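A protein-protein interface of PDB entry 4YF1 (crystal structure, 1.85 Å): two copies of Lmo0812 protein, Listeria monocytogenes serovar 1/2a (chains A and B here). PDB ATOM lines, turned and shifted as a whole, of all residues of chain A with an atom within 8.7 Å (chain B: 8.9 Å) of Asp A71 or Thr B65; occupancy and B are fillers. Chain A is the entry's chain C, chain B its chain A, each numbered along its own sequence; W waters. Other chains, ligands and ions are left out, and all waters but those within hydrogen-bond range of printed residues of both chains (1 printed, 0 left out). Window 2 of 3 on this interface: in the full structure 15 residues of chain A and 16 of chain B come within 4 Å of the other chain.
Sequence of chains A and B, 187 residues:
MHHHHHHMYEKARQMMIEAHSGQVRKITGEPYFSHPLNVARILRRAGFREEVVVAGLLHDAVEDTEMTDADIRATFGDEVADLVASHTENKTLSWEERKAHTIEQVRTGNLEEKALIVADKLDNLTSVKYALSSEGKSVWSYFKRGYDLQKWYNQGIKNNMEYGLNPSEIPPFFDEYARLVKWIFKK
The backbone carbonyl oxygen of Ala B61 sits at hydrogen-bond distance from the side-chain hydroxyl of Thr B65.
The side-chain hydroxyl (OG1) of Thr B65 lies close to the backbone NH (N) of Met B67 (3.1 Å).
N of Thr B68 sits at hydrogen-bond distance from OD2 of Asp B71, at 3.0 Å.
The side-chain hydroxyl of Thr A68 is in hydrogen-bond range of the backbone NH of Asp A71 (3.1 Å).
OG1 of Thr A75 sits at hydrogen-bond distance from O of Asp A71, 2.9 Å away.
Among the printed residues, pairs that only touch across the chains: Thr A65 with Asp B71 (3.7 Å), Asp A71 with Thr B65 (3.96 Å), Thr A75 with Pro B36 (3.3 Å), Thr A75 with Asp B60 (3.9 Å), Thr A75 with Ala B61 (3.9 Å), Thr A75 with Thr B65 (3.4 Å) and Phe A76 with Pro B36 (3.9 Å).
Of chain B, only Thr B65 (3.96 Å) comes within 4 Å of Asp A71.
Thr B65 touches just these residues of chain A: Asp A71 (3.96 Å) and Thr A75 (3.4 Å).
Ala A70 touches none of the printed residues of chain B.
Of the printed residues of chain A, Pro B36 touches Thr A75 and Phe A76.
Of the printed residues of chain B, Phe A76 touches Pro B36 (3.9 Å).
Of the printed residues of chain A, Asp B71 touches Thr A65 (3.7 Å).
Printed residues of chain A within 4 Å of Asp B60: Thr A75.
Of the printed residues of chain B, Thr A65 touches Asp B71.
Thr A68 touches none of the printed residues of chain B.
Met A67 touches none of the printed residues of chain B.
The nearest residue of chain B that does not touch Asp A71 is Glu B66 (4.8 Å).
Printed residues of chain A that touch a printed residue of chain B: Thr A65, Asp A71, Thr A75 and Phe A76.
Hydrophobic or aromatic side chains of chain A that line the printed part of chain B: Phe A76.
Of the 16 printed residues of chain B, 5 touch a printed residue of chain A.
Among the printed residues, 7 pairs touch across the chains.
Among the printed residues, no Asp or Glu carboxylate lies within 4 Å of a Lys or Arg side-chain nitrogen of the other chain.
Thr A65 touches Asp B71, and with the chains exchanged Asp A71 touches Thr B65.
Positions printed for both chains: 58, 62, 65, 66, 67, 68, 69, 71 and 72.
Of the 7 pairs that touch across the chains among the printed residues, 2 have their exchanged pair printed and touching as well.
Water W1 lies within hydrogen-bond range of OD2 of Asp B60 (2.8 Å) and O of Thr A75 (2.8 Å).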
ATOM      1  N   LEU A  58     -26.583  32.493  23.120  1.00  0.00           N
ATOM      2  CA  LEU A  58     -26.212  32.855  21.759  1.00  0.00           C
ATOM      3  C   LEU A  58     -25.520  34.186  21.562  1.00  0.00           C
ATOM      4  O   LEU A  58     -24.946  34.408  20.503  1.00  0.00           O
ATOM      5  CB  LEU A  58     -27.459  32.826  20.844  1.00  0.00           C
ATOM      6  CG  LEU A  58     -28.090  31.468  20.545  1.00  0.00           C
ATOM      7  CD1 LEU A  58     -29.309  31.682  19.644  1.00  0.00           C
ATOM      8  CD2 LEU A  58     -27.091  30.543  19.871  1.00  0.00           C
ATOM      9  N   VAL A  62     -23.453  35.128  18.142  1.00  0.00           N
ATOM     10  CA  VAL A  62     -24.089  36.081  17.225  1.00  0.00           C
ATOM     11  C   VAL A  62     -23.158  37.232  16.891  1.00  0.00           C
ATOM     12  O   VAL A  62     -23.046  37.606  15.724  1.00  0.00           O
ATOM     13  CB  VAL A  62     -25.436  36.610  17.791  1.00  0.00           C
ATOM     14  CG1 VAL A  62     -25.987  37.764  16.958  1.00  0.00           C
ATOM     15  CG2 VAL A  62     -26.447  35.471  17.856  1.00  0.00           C
ATOM     16  N   THR A  65     -19.776  36.005  14.910  1.00  0.00           N
ATOM     17  CA  THR A  65     -20.014  35.572  13.526  1.00  0.00           C
ATOM     18  C   THR A  65     -20.904  36.533  12.744  1.00  0.00           C
ATOM     19  O   THR A  65     -21.170  36.297  11.563  1.00  0.00           O
ATOM     20  CB  THR A  65     -20.706  34.196  13.487  1.00  0.00           C
ATOM     21  OG1 THR A  65     -22.044  34.298  14.004  1.00  0.00           O
ATOM     22  CG2 THR A  65     -19.916  33.172  14.289  1.00  0.00           C
ATOM     23  N   GLU A  66     -21.379  37.592  13.402  1.00  0.00           N
ATOM     24  CA  GLU A  66     -22.284  38.559  12.771  1.00  0.00           C
ATOM     25  C   GLU A  66     -23.461  37.848  12.077  1.00  0.00           C
ATOM     26  O   GLU A  66     -23.757  38.095  10.901  1.00  0.00           O
ATOM     27  CB  GLU A  66     -21.518  39.457  11.785  1.00  0.00           C
ATOM     28  CG  GLU A  66     -20.422  40.283  12.440  1.00  0.00           C
ATOM     29  CD  GLU A  66     -19.694  41.195  11.464  1.00  0.00           C
ATOM     30  OE1 GLU A  66     -19.417  40.764  10.317  1.00  0.00           O
ATOM     31  OE2 GLU A  66     -19.367  42.337  11.856  1.00  0.00           O
ATOM     32  N   MET A  67     -24.098  36.942  12.813  1.00  0.00           N
ATOM     33  CA  MET A  67     -25.237  36.192  12.299  1.00  0.00           C
ATOM     34  C   MET A  67     -26.356  37.177  12.198  1.00  0.00           C
ATOM     35  O   MET A  67     -26.586  37.945  13.126  1.00  0.00           O
ATOM     36  CB  MET A  67     -25.608  35.052  13.257  1.00  0.00           C
ATOM     37  CG  MET A  67     -26.260  33.885  12.519  1.00  0.00           C
ATOM     38  SD  MET A  67     -27.100  32.590  13.755  1.00  0.00           S
ATOM     39  CE  MET A  67     -25.792  32.588  15.230  1.00  0.00           C
ATOM     40  N   THR A  68     -27.051  37.174  11.070  1.00  0.00           N
ATOM     41  CA  THR A  68     -28.147  38.107  10.843  1.00  0.00           C
ATOM     42  C   THR A  68     -29.378  37.758  11.662  1.00  0.00           C
ATOM     43  O   THR A  68     -29.509  36.644  12.177  1.00  0.00           O
ATOM     44  CB  THR A  68     -28.582  38.104   9.373  1.00  0.00           C
ATOM     45  OG1 THR A  68     -29.044  36.791   9.013  1.00  0.00           O
ATOM     46  CG2 THR A  68     -27.423  38.503   8.479  1.00  0.00           C
ATOM     47  N   ASP A  69     -30.276  38.727  11.768  1.00  0.00           N
ATOM     48  CA  ASP A  69     -31.526  38.542  12.462  1.00  0.00           C
ATOM     49  C   ASP A  69     -32.312  37.459  11.740  1.00  0.00           C
ATOM     50  O   ASP A  69     -32.881  36.577  12.374  1.00  0.00           O
ATOM     51  CB  ASP A  69     -32.340  39.832  12.470  1.00  0.00           C
ATOM     52  CG  ASP A  69     -33.626  39.694  13.247  1.00  0.00           C
ATOM     53  OD1 ASP A  69     -33.564  39.685  14.495  1.00  0.00           O
ATOM     54  OD2 ASP A  69     -34.701  39.611  12.617  1.00  0.00           O
ATOM     55  N   ALA A  70     -32.325  37.533  10.408  1.00  0.00           N
ATOM     56  CA  ALA A  70     -33.025  36.552   9.580  1.00  0.00           C
ATOM     57  C   ALA A  70     -32.558  35.119   9.868  1.00  0.00           C
ATOM     58  O   ALA A  70     -33.383  34.207   9.953  1.00  0.00           O
ATOM     59  CB  ALA A  70     -32.856  36.884   8.107  1.00  0.00           C
ATOM     60  N   ASP A  71     -31.245  34.923  10.017  1.00  0.00           N
ATOM     61  CA  ASP A  71     -30.712  33.594  10.348  1.00  0.00           C
ATOM     62  C   ASP A  71     -31.145  33.145  11.747  1.00  0.00           C
ATOM     63  O   ASP A  71     -31.575  32.004  11.921  1.00  0.00           O
ATOM     64  CB  ASP A  71     -29.179  33.532  10.230  1.00  0.00           C
ATOM     65  CG  ASP A  71     -28.690  33.244   8.803  1.00  0.00           C
ATOM     66  OD1 ASP A  71     -29.505  32.888   7.915  1.00  0.00           O
ATOM     67  OD2 ASP A  71     -27.462  33.337   8.584  1.00  0.00           O
ATOM     68  N   ILE A  72     -31.027  34.030  12.733  1.00  0.00           N
ATOM     69  CA  ILE A  72     -31.426  33.687  14.104  1.00  0.00           C
ATOM     70  C   ILE A  72     -32.913  33.365  14.134  1.00  0.00           C
ATOM     71  O   ILE A  72     -33.322  32.365  14.699  1.00  0.00           O
ATOM     72  CB  ILE A  72     -31.137  34.829  15.094  1.00  0.00           C
ATOM     73  CG1 ILE A  72     -29.636  35.145  15.131  1.00  0.00           C
ATOM     74  CG2 ILE A  72     -31.614  34.443  16.486  1.00  0.00           C
ATOM     75  CD1 ILE A  72     -29.319  36.509  15.715  1.00  0.00           C
ATOM     76  N   ARG A  73     -33.695  34.221  13.487  1.00  0.00           N
ATOM     77  CA  ARG A  73     -35.145  34.089  13.410  1.00  0.00           C
ATOM     78  C   ARG A  73     -35.591  32.788  12.705  1.00  0.00           C
ATOM     79  O   ARG A  73     -36.485  32.079  13.199  1.00  0.00           O
ATOM     80  CB  ARG A  73     -35.717  35.337  12.718  1.00  0.00           C
ATOM     81  CG  ARG A  73     -37.228  35.504  12.793  1.00  0.00           C
ATOM     82  CD  ARG A  73     -37.659  36.910  12.355  1.00  0.00           C
ATOM     83  NE  ARG A  73     -37.038  37.982  13.153  1.00  0.00           N
ATOM     84  CZ  ARG A  73     -37.452  38.405  14.354  1.00  0.00           C
ATOM     85  NH1 ARG A  73     -38.503  37.849  14.960  1.00  0.00           N
ATOM     86  NH2 ARG A  73     -36.800  39.390  14.968  1.00  0.00           N
ATOM     87  N   ALA A  74     -34.964  32.459  11.576  1.00  0.00           N
ATOM     88  CA  ALA A  74     -35.329  31.229  10.838  1.00  0.00           C
ATOM     89  C   ALA A  74     -34.873  29.953  11.556  1.00  0.00           C
ATOM     90  O   ALA A  74     -35.519  28.914  11.447  1.00  0.00           O
ATOM     91  CB  ALA A  74     -34.772  31.263   9.429  1.00  0.00           C
ATOM     92  N   THR A  75     -33.786  30.039  12.318  1.00  0.00           N
ATOM     93  CA  THR A  75     -33.263  28.866  12.993  1.00  0.00           C
ATOM     94  C   THR A  75     -33.891  28.656  14.383  1.00  0.00           C
ATOM     95  O   THR A  75     -34.359  27.576  14.685  1.00  0.00           O
ATOM     96  CB  THR A  75     -31.730  28.948  13.143  1.00  0.00           C
ATOM     97  OG1 THR A  75     -31.132  29.156  11.860  1.00  0.00           O
ATOM     98  CG2 THR A  75     -31.172  27.654  13.725  1.00  0.00           C
ATOM     99  N   PHE A  76     -33.915  29.708  15.188  1.00  0.00           N
ATOM    100  CA  PHE A  76     -34.359  29.622  16.560  1.00  0.00           C
ATOM    101  C   PHE A  76     -35.751  30.151  16.905  1.00  0.00           C
ATOM    102  O   PHE A  76     -36.215  29.945  18.040  1.00  0.00           O
ATOM    103  CB  PHE A  76     -33.320  30.317  17.438  1.00  0.00           C
ATOM    104  CG  PHE A  76     -31.974  29.710  17.329  1.00  0.00           C
ATOM    105  CD1 PHE A  76     -31.708  28.485  17.935  1.00  0.00           C
ATOM    106  CD2 PHE A  76     -30.970  30.338  16.620  1.00  0.00           C
ATOM    107  CE1 PHE A  76     -30.453  27.910  17.829  1.00  0.00           C
ATOM    108  CE2 PHE A  76     -29.697  29.766  16.526  1.00  0.00           C
ATOM    109  CZ  PHE A  76     -29.442  28.550  17.130  1.00  0.00           C
ATOM    110  N   GLY A  77     -36.408  30.830  15.964  1.00  0.00           N
ATOM    111  CA  GLY A  77     -37.737  31.369  16.204  1.00  0.00           C
ATOM    112  C   GLY A  77     -37.755  32.854  16.515  1.00  0.00           C
ATOM    113  O   GLY A  77     -36.729  33.446  16.866  1.00  0.00           O
ATOM    114  N   VAL A  80     -36.728  34.124  20.415  1.00  0.00           N
ATOM    115  CA  VAL A  80     -35.270  34.182  20.609  1.00  0.00           C
ATOM    116  C   VAL A  80     -34.682  35.373  19.845  1.00  0.00           C
ATOM    117  O   VAL A  80     -33.916  36.172  20.401  1.00  0.00           O
ATOM    118  CB  VAL A  80     -34.605  32.884  20.130  1.00  0.00           C
ATOM    119  CG1 VAL A  80     -33.082  33.004  20.123  1.00  0.00           C
ATOM    120  CG2 VAL A  80     -35.052  31.725  20.997  1.00  0.00           C
ATOM    121  N   ALA A  81     -35.071  35.496  18.573  1.00  0.00           N
ATOM    122  CA  ALA A  81     -34.584  36.570  17.711  1.00  0.00           C
ATOM    123  C   ALA A  81     -34.813  37.972  18.302  1.00  0.00           C
ATOM    124  O   ALA A  81     -33.911  38.818  18.284  1.00  0.00           O
ATOM    125  CB  ALA A  81     -35.217  36.462  16.335  1.00  0.00           C
ATOM    126  N   PRO B  36     -34.793  23.542  17.157  1.00  0.00           N
ATOM    127  CA  PRO B  36     -33.695  23.502  18.151  1.00  0.00           C
ATOM    128  C   PRO B  36     -34.167  23.602  19.603  1.00  0.00           C
ATOM    129  O   PRO B  36     -33.631  22.894  20.447  1.00  0.00           O
ATOM    130  CB  PRO B  36     -32.851  24.722  17.795  1.00  0.00           C
ATOM    131  CG  PRO B  36     -33.133  24.981  16.356  1.00  0.00           C
ATOM    132  CD  PRO B  36     -34.585  24.632  16.176  1.00  0.00           C
ATOM    133  N   LEU B  58     -27.639  23.573  18.640  1.00  0.00           N
ATOM    134  CA  LEU B  58     -26.819  24.108  17.542  1.00  0.00           C
ATOM    135  C   LEU B  58     -26.825  23.300  16.236  1.00  0.00           C
ATOM    136  O   LEU B  58     -26.324  23.780  15.218  1.00  0.00           O
ATOM    137  CB  LEU B  58     -25.395  24.303  18.024  1.00  0.00           C
ATOM    138  CG  LEU B  58     -25.242  25.329  19.153  1.00  0.00           C
ATOM    139  CD1 LEU B  58     -23.820  25.310  19.687  1.00  0.00           C
ATOM    140  CD2 LEU B  58     -25.613  26.731  18.696  1.00  0.00           C
ATOM    141  N   HIS B  59     -27.402  22.103  16.255  1.00  0.00           N
ATOM    142  CA  HIS B  59     -27.426  21.261  15.062  1.00  0.00           C
ATOM    143  C   HIS B  59     -27.920  22.001  13.801  1.00  0.00           C
ATOM    144  O   HIS B  59     -27.206  22.034  12.792  1.00  0.00           O
ATOM    145  CB  HIS B  59     -28.216  19.969  15.340  1.00  0.00           C
ATOM    146  CG  HIS B  59     -28.501  19.150  14.120  1.00  0.00           C
ATOM    147  ND1 HIS B  59     -27.622  18.213  13.625  1.00  0.00           N
ATOM    148  CD2 HIS B  59     -29.573  19.137  13.288  1.00  0.00           C
ATOM    149  CE1 HIS B  59     -28.139  17.654  12.541  1.00  0.00           C
ATOM    150  NE2 HIS B  59     -29.327  18.189  12.324  1.00  0.00           N
ATOM    151  N   ASP B  60     -29.107  22.605  13.867  1.00  0.00           N
ATOM    152  CA  ASP B  60     -29.677  23.348  12.703  1.00  0.00           C
ATOM    153  C   ASP B  60     -28.864  24.579  12.312  1.00  0.00           C
ATOM    154  O   ASP B  60     -28.860  24.965  11.143  1.00  0.00           O
ATOM    155  CB  ASP B  60     -31.103  23.845  12.980  1.00  0.00           C
ATOM    156  CG  ASP B  60     -32.139  22.741  12.999  1.00  0.00           C
ATOM    157  OD1 ASP B  60     -31.806  21.535  12.869  1.00  0.00           O
ATOM    158  OD2 ASP B  60     -33.323  23.110  13.137  1.00  0.00           O
ATOM    159  N   ALA B  61     -28.203  25.201  13.291  1.00  0.00           N
ATOM    160  CA  ALA B  61     -27.386  26.392  13.030  1.00  0.00           C
ATOM    161  C   ALA B  61     -26.234  26.056  12.090  1.00  0.00           C
ATOM    162  O   ALA B  61     -25.923  26.827  11.172  1.00  0.00           O
ATOM    163  CB  ALA B  61     -26.853  26.971  14.325  1.00  0.00           C
ATOM    164  N   VAL B  62     -25.608  24.897  12.308  1.00  0.00           N
ATOM    165  CA  VAL B  62     -24.490  24.470  11.464  1.00  0.00           C
ATOM    166  C   VAL B  62     -24.975  23.996  10.101  1.00  0.00           C
ATOM    167  O   VAL B  62     -24.411  24.393   9.074  1.00  0.00           O
ATOM    168  CB  VAL B  62     -23.685  23.322  12.087  1.00  0.00           C
ATOM    169  CG1 VAL B  62     -22.525  22.931  11.170  1.00  0.00           C
ATOM    170  CG2 VAL B  62     -23.156  23.737  13.431  1.00  0.00           C
ATOM    171  N   GLU B  63     -25.986  23.129  10.087  1.00  0.00           N
ATOM    172  CA  GLU B  63     -26.510  22.600   8.813  1.00  0.00           C
ATOM    173  C   GLU B  63     -27.281  23.608   7.945  1.00  0.00           C
ATOM    174  O   GLU B  63     -27.175  23.553   6.712  1.00  0.00           O
ATOM    175  CB  GLU B  63     -27.383  21.352   9.034  1.00  0.00           C
ATOM    176  CG  GLU B  63     -26.617  20.138   9.552  1.00  0.00           C
ATOM    177  CD  GLU B  63     -27.349  18.815   9.331  1.00  0.00           C
ATOM    178  OE1 GLU B  63     -26.670  17.771   9.449  1.00  0.00           O
ATOM    179  OE2 GLU B  63     -28.580  18.805   9.013  1.00  0.00           O
ATOM    180  N   ASP B  64     -28.033  24.521   8.566  1.00  0.00           N
ATOM    181  CA  ASP B  64     -28.894  25.456   7.801  1.00  0.00           C
ATOM    182  C   ASP B  64     -28.362  26.878   7.612  1.00  0.00           C
ATOM    183  O   ASP B  64     -28.949  27.635   6.849  1.00  0.00           O
ATOM    184  CB  ASP B  64     -30.310  25.506   8.408  1.00  0.00           C
ATOM    185  CG  ASP B  64     -30.970  24.119   8.492  1.00  0.00           C
ATOM    186  OD1 ASP B  64     -30.593  23.223   7.704  1.00  0.00           O
ATOM    187  OD2 ASP B  64     -31.869  23.919   9.345  1.00  0.00           O
ATOM    188  N   THR B  65     -27.282  27.249   8.301  1.00  0.00           N
ATOM    189  CA  THR B  65     -26.707  28.597   8.151  1.00  0.00           C
ATOM    190  C   THR B  65     -25.220  28.481   7.848  1.00  0.00           C
ATOM    191  O   THR B  65     -24.650  27.375   7.874  1.00  0.00           O
ATOM    192  CB  THR B  65     -26.916  29.497   9.401  1.00  0.00           C
ATOM    193  OG1 THR B  65     -25.893  29.278  10.382  1.00  0.00           O
ATOM    194  CG2 THR B  65     -28.302  29.280  10.016  1.00  0.00           C
ATOM    195  N   GLU B  66     -24.584  29.619   7.591  1.00  0.00           N
ATOM    196  CA  GLU B  66     -23.155  29.645   7.273  1.00  0.00           C
ATOM    197  C   GLU B  66     -22.261  29.432   8.486  1.00  0.00           C
ATOM    198  O   GLU B  66     -21.050  29.355   8.339  1.00  0.00           O
ATOM    199  CB  GLU B  66     -22.774  30.939   6.534  1.00  0.00           C
ATOM    200  CG  GLU B  66     -23.439  31.115   5.171  1.00  0.00           C
ATOM    201  CD  GLU B  66     -23.148  29.974   4.193  1.00  0.00           C
ATOM    202  OE1 GLU B  66     -22.403  30.202   3.215  1.00  0.00           O
ATOM    203  OE2 GLU B  66     -23.631  28.836   4.411  1.00  0.00           O
ATOM    204  N   MET B  67     -22.846  29.315   9.676  1.00  0.00           N
ATOM    205  CA  MET B  67     -22.053  29.027  10.879  1.00  0.00           C
ATOM    206  C   MET B  67     -21.347  27.708  10.637  1.00  0.00           C
ATOM    207  O   MET B  67     -21.925  26.777  10.052  1.00  0.00           O
ATOM    208  CB  MET B  67     -22.937  28.975  12.128  1.00  0.00           C
ATOM    209  CG  MET B  67     -22.128  28.798  13.407  1.00  0.00           C
ATOM    210  SD  MET B  67     -23.308  28.908  14.995  1.00  0.00           S
ATOM    211  CE  MET B  67     -21.996  29.815  16.154  1.00  0.00           C
ATOM    212  N   THR B  68     -20.098  27.619  11.088  1.00  0.00           N
ATOM    213  CA  THR B  68     -19.252  26.446  10.867  1.00  0.00           C
ATOM    214  C   THR B  68     -18.775  25.780  12.154  1.00  0.00           C
ATOM    215  O   THR B  68     -18.966  26.302  13.253  1.00  0.00           O
ATOM    216  CB  THR B  68     -17.974  26.871  10.127  1.00  0.00           C
ATOM    217  OG1 THR B  68     -17.174  27.703  10.988  1.00  0.00           O
ATOM    218  CG2 THR B  68     -18.315  27.627   8.848  1.00  0.00           C
ATOM    219  N   ASP B  69     -18.106  24.639  11.984  1.00  0.00           N
ATOM    220  CA  ASP B  69     -17.484  23.920  13.086  1.00  0.00           C
ATOM    221  C   ASP B  69     -16.494  24.828  13.839  1.00  0.00           C
ATOM    222  O   ASP B  69     -16.441  24.817  15.071  1.00  0.00           O
ATOM    223  CB  ASP B  69     -16.714  22.704  12.544  1.00  0.00           C
ATOM    224  CG  ASP B  69     -15.945  21.975  13.629  1.00  0.00           C
ATOM    225  OD1 ASP B  69     -16.543  21.171  14.367  1.00  0.00           O
ATOM    226  OD2 ASP B  69     -14.733  22.194  13.740  1.00  0.00           O
ATOM    227  N   ASP B  71     -16.497  28.120  14.077  1.00  0.00           N
ATOM    228  CA  ASP B  71     -17.262  29.123  14.852  1.00  0.00           C
ATOM    229  C   ASP B  71     -17.741  28.518  16.180  1.00  0.00           C
ATOM    230  O   ASP B  71     -17.618  29.147  17.233  1.00  0.00           O
ATOM    231  CB  ASP B  71     -18.476  29.626  14.072  1.00  0.00           C
ATOM    232  CG  ASP B  71     -18.107  30.362  12.795  1.00  0.00           C
ATOM    233  OD1 ASP B  71     -17.094  31.096  12.789  1.00  0.00           O
ATOM    234  OD2 ASP B  71     -18.862  30.236  11.802  1.00  0.00           O
ATOM    235  N   ILE B  72     -18.278  27.294  16.140  1.00  0.00           N
ATOM    236  CA  ILE B  72     -18.725  26.646  17.387  1.00  0.00           C
ATOM    237  C   ILE B  72     -17.571  26.432  18.366  1.00  0.00           C
ATOM    238  O   ILE B  72     -17.732  26.686  19.554  1.00  0.00           O
ATOM    239  CB  ILE B  72     -19.463  25.319  17.125  1.00  0.00           C
ATOM    240  CG1 ILE B  72     -20.727  25.618  16.318  1.00  0.00           C
ATOM    241  CG2 ILE B  72     -19.848  24.633  18.442  1.00  0.00           C
ATOM    242  CD1 ILE B  72     -21.556  24.409  16.002  1.00  0.00           C
ATOM    243  N   LYS B  91     -22.934  17.556   3.571  1.00  0.00           N
ATOM    244  CA  LYS B  91     -23.909  17.942   2.522  1.00  0.00           C
ATOM    245  C   LYS B  91     -23.491  17.631   1.080  1.00  0.00           C
ATOM    246  O   LYS B  91     -24.330  17.685   0.175  1.00  0.00           O
ATOM    247  CB  LYS B  91     -24.201  19.443   2.596  1.00  0.00           C
ATOM    248  CG  LYS B  91     -24.589  20.017   3.956  1.00  0.00           C
ATOM    249  CD  LYS B  91     -26.050  19.869   4.357  1.00  0.00           C
ATOM    250  CE  LYS B  91     -26.460  18.461   4.746  1.00  0.00           C
ATOM    251  NZ  LYS B  91     -27.713  18.523   5.563  1.00  0.00           N
HETATM  252  O   HOH W   1     -34.482  25.571  12.676  1.00  0.00           O
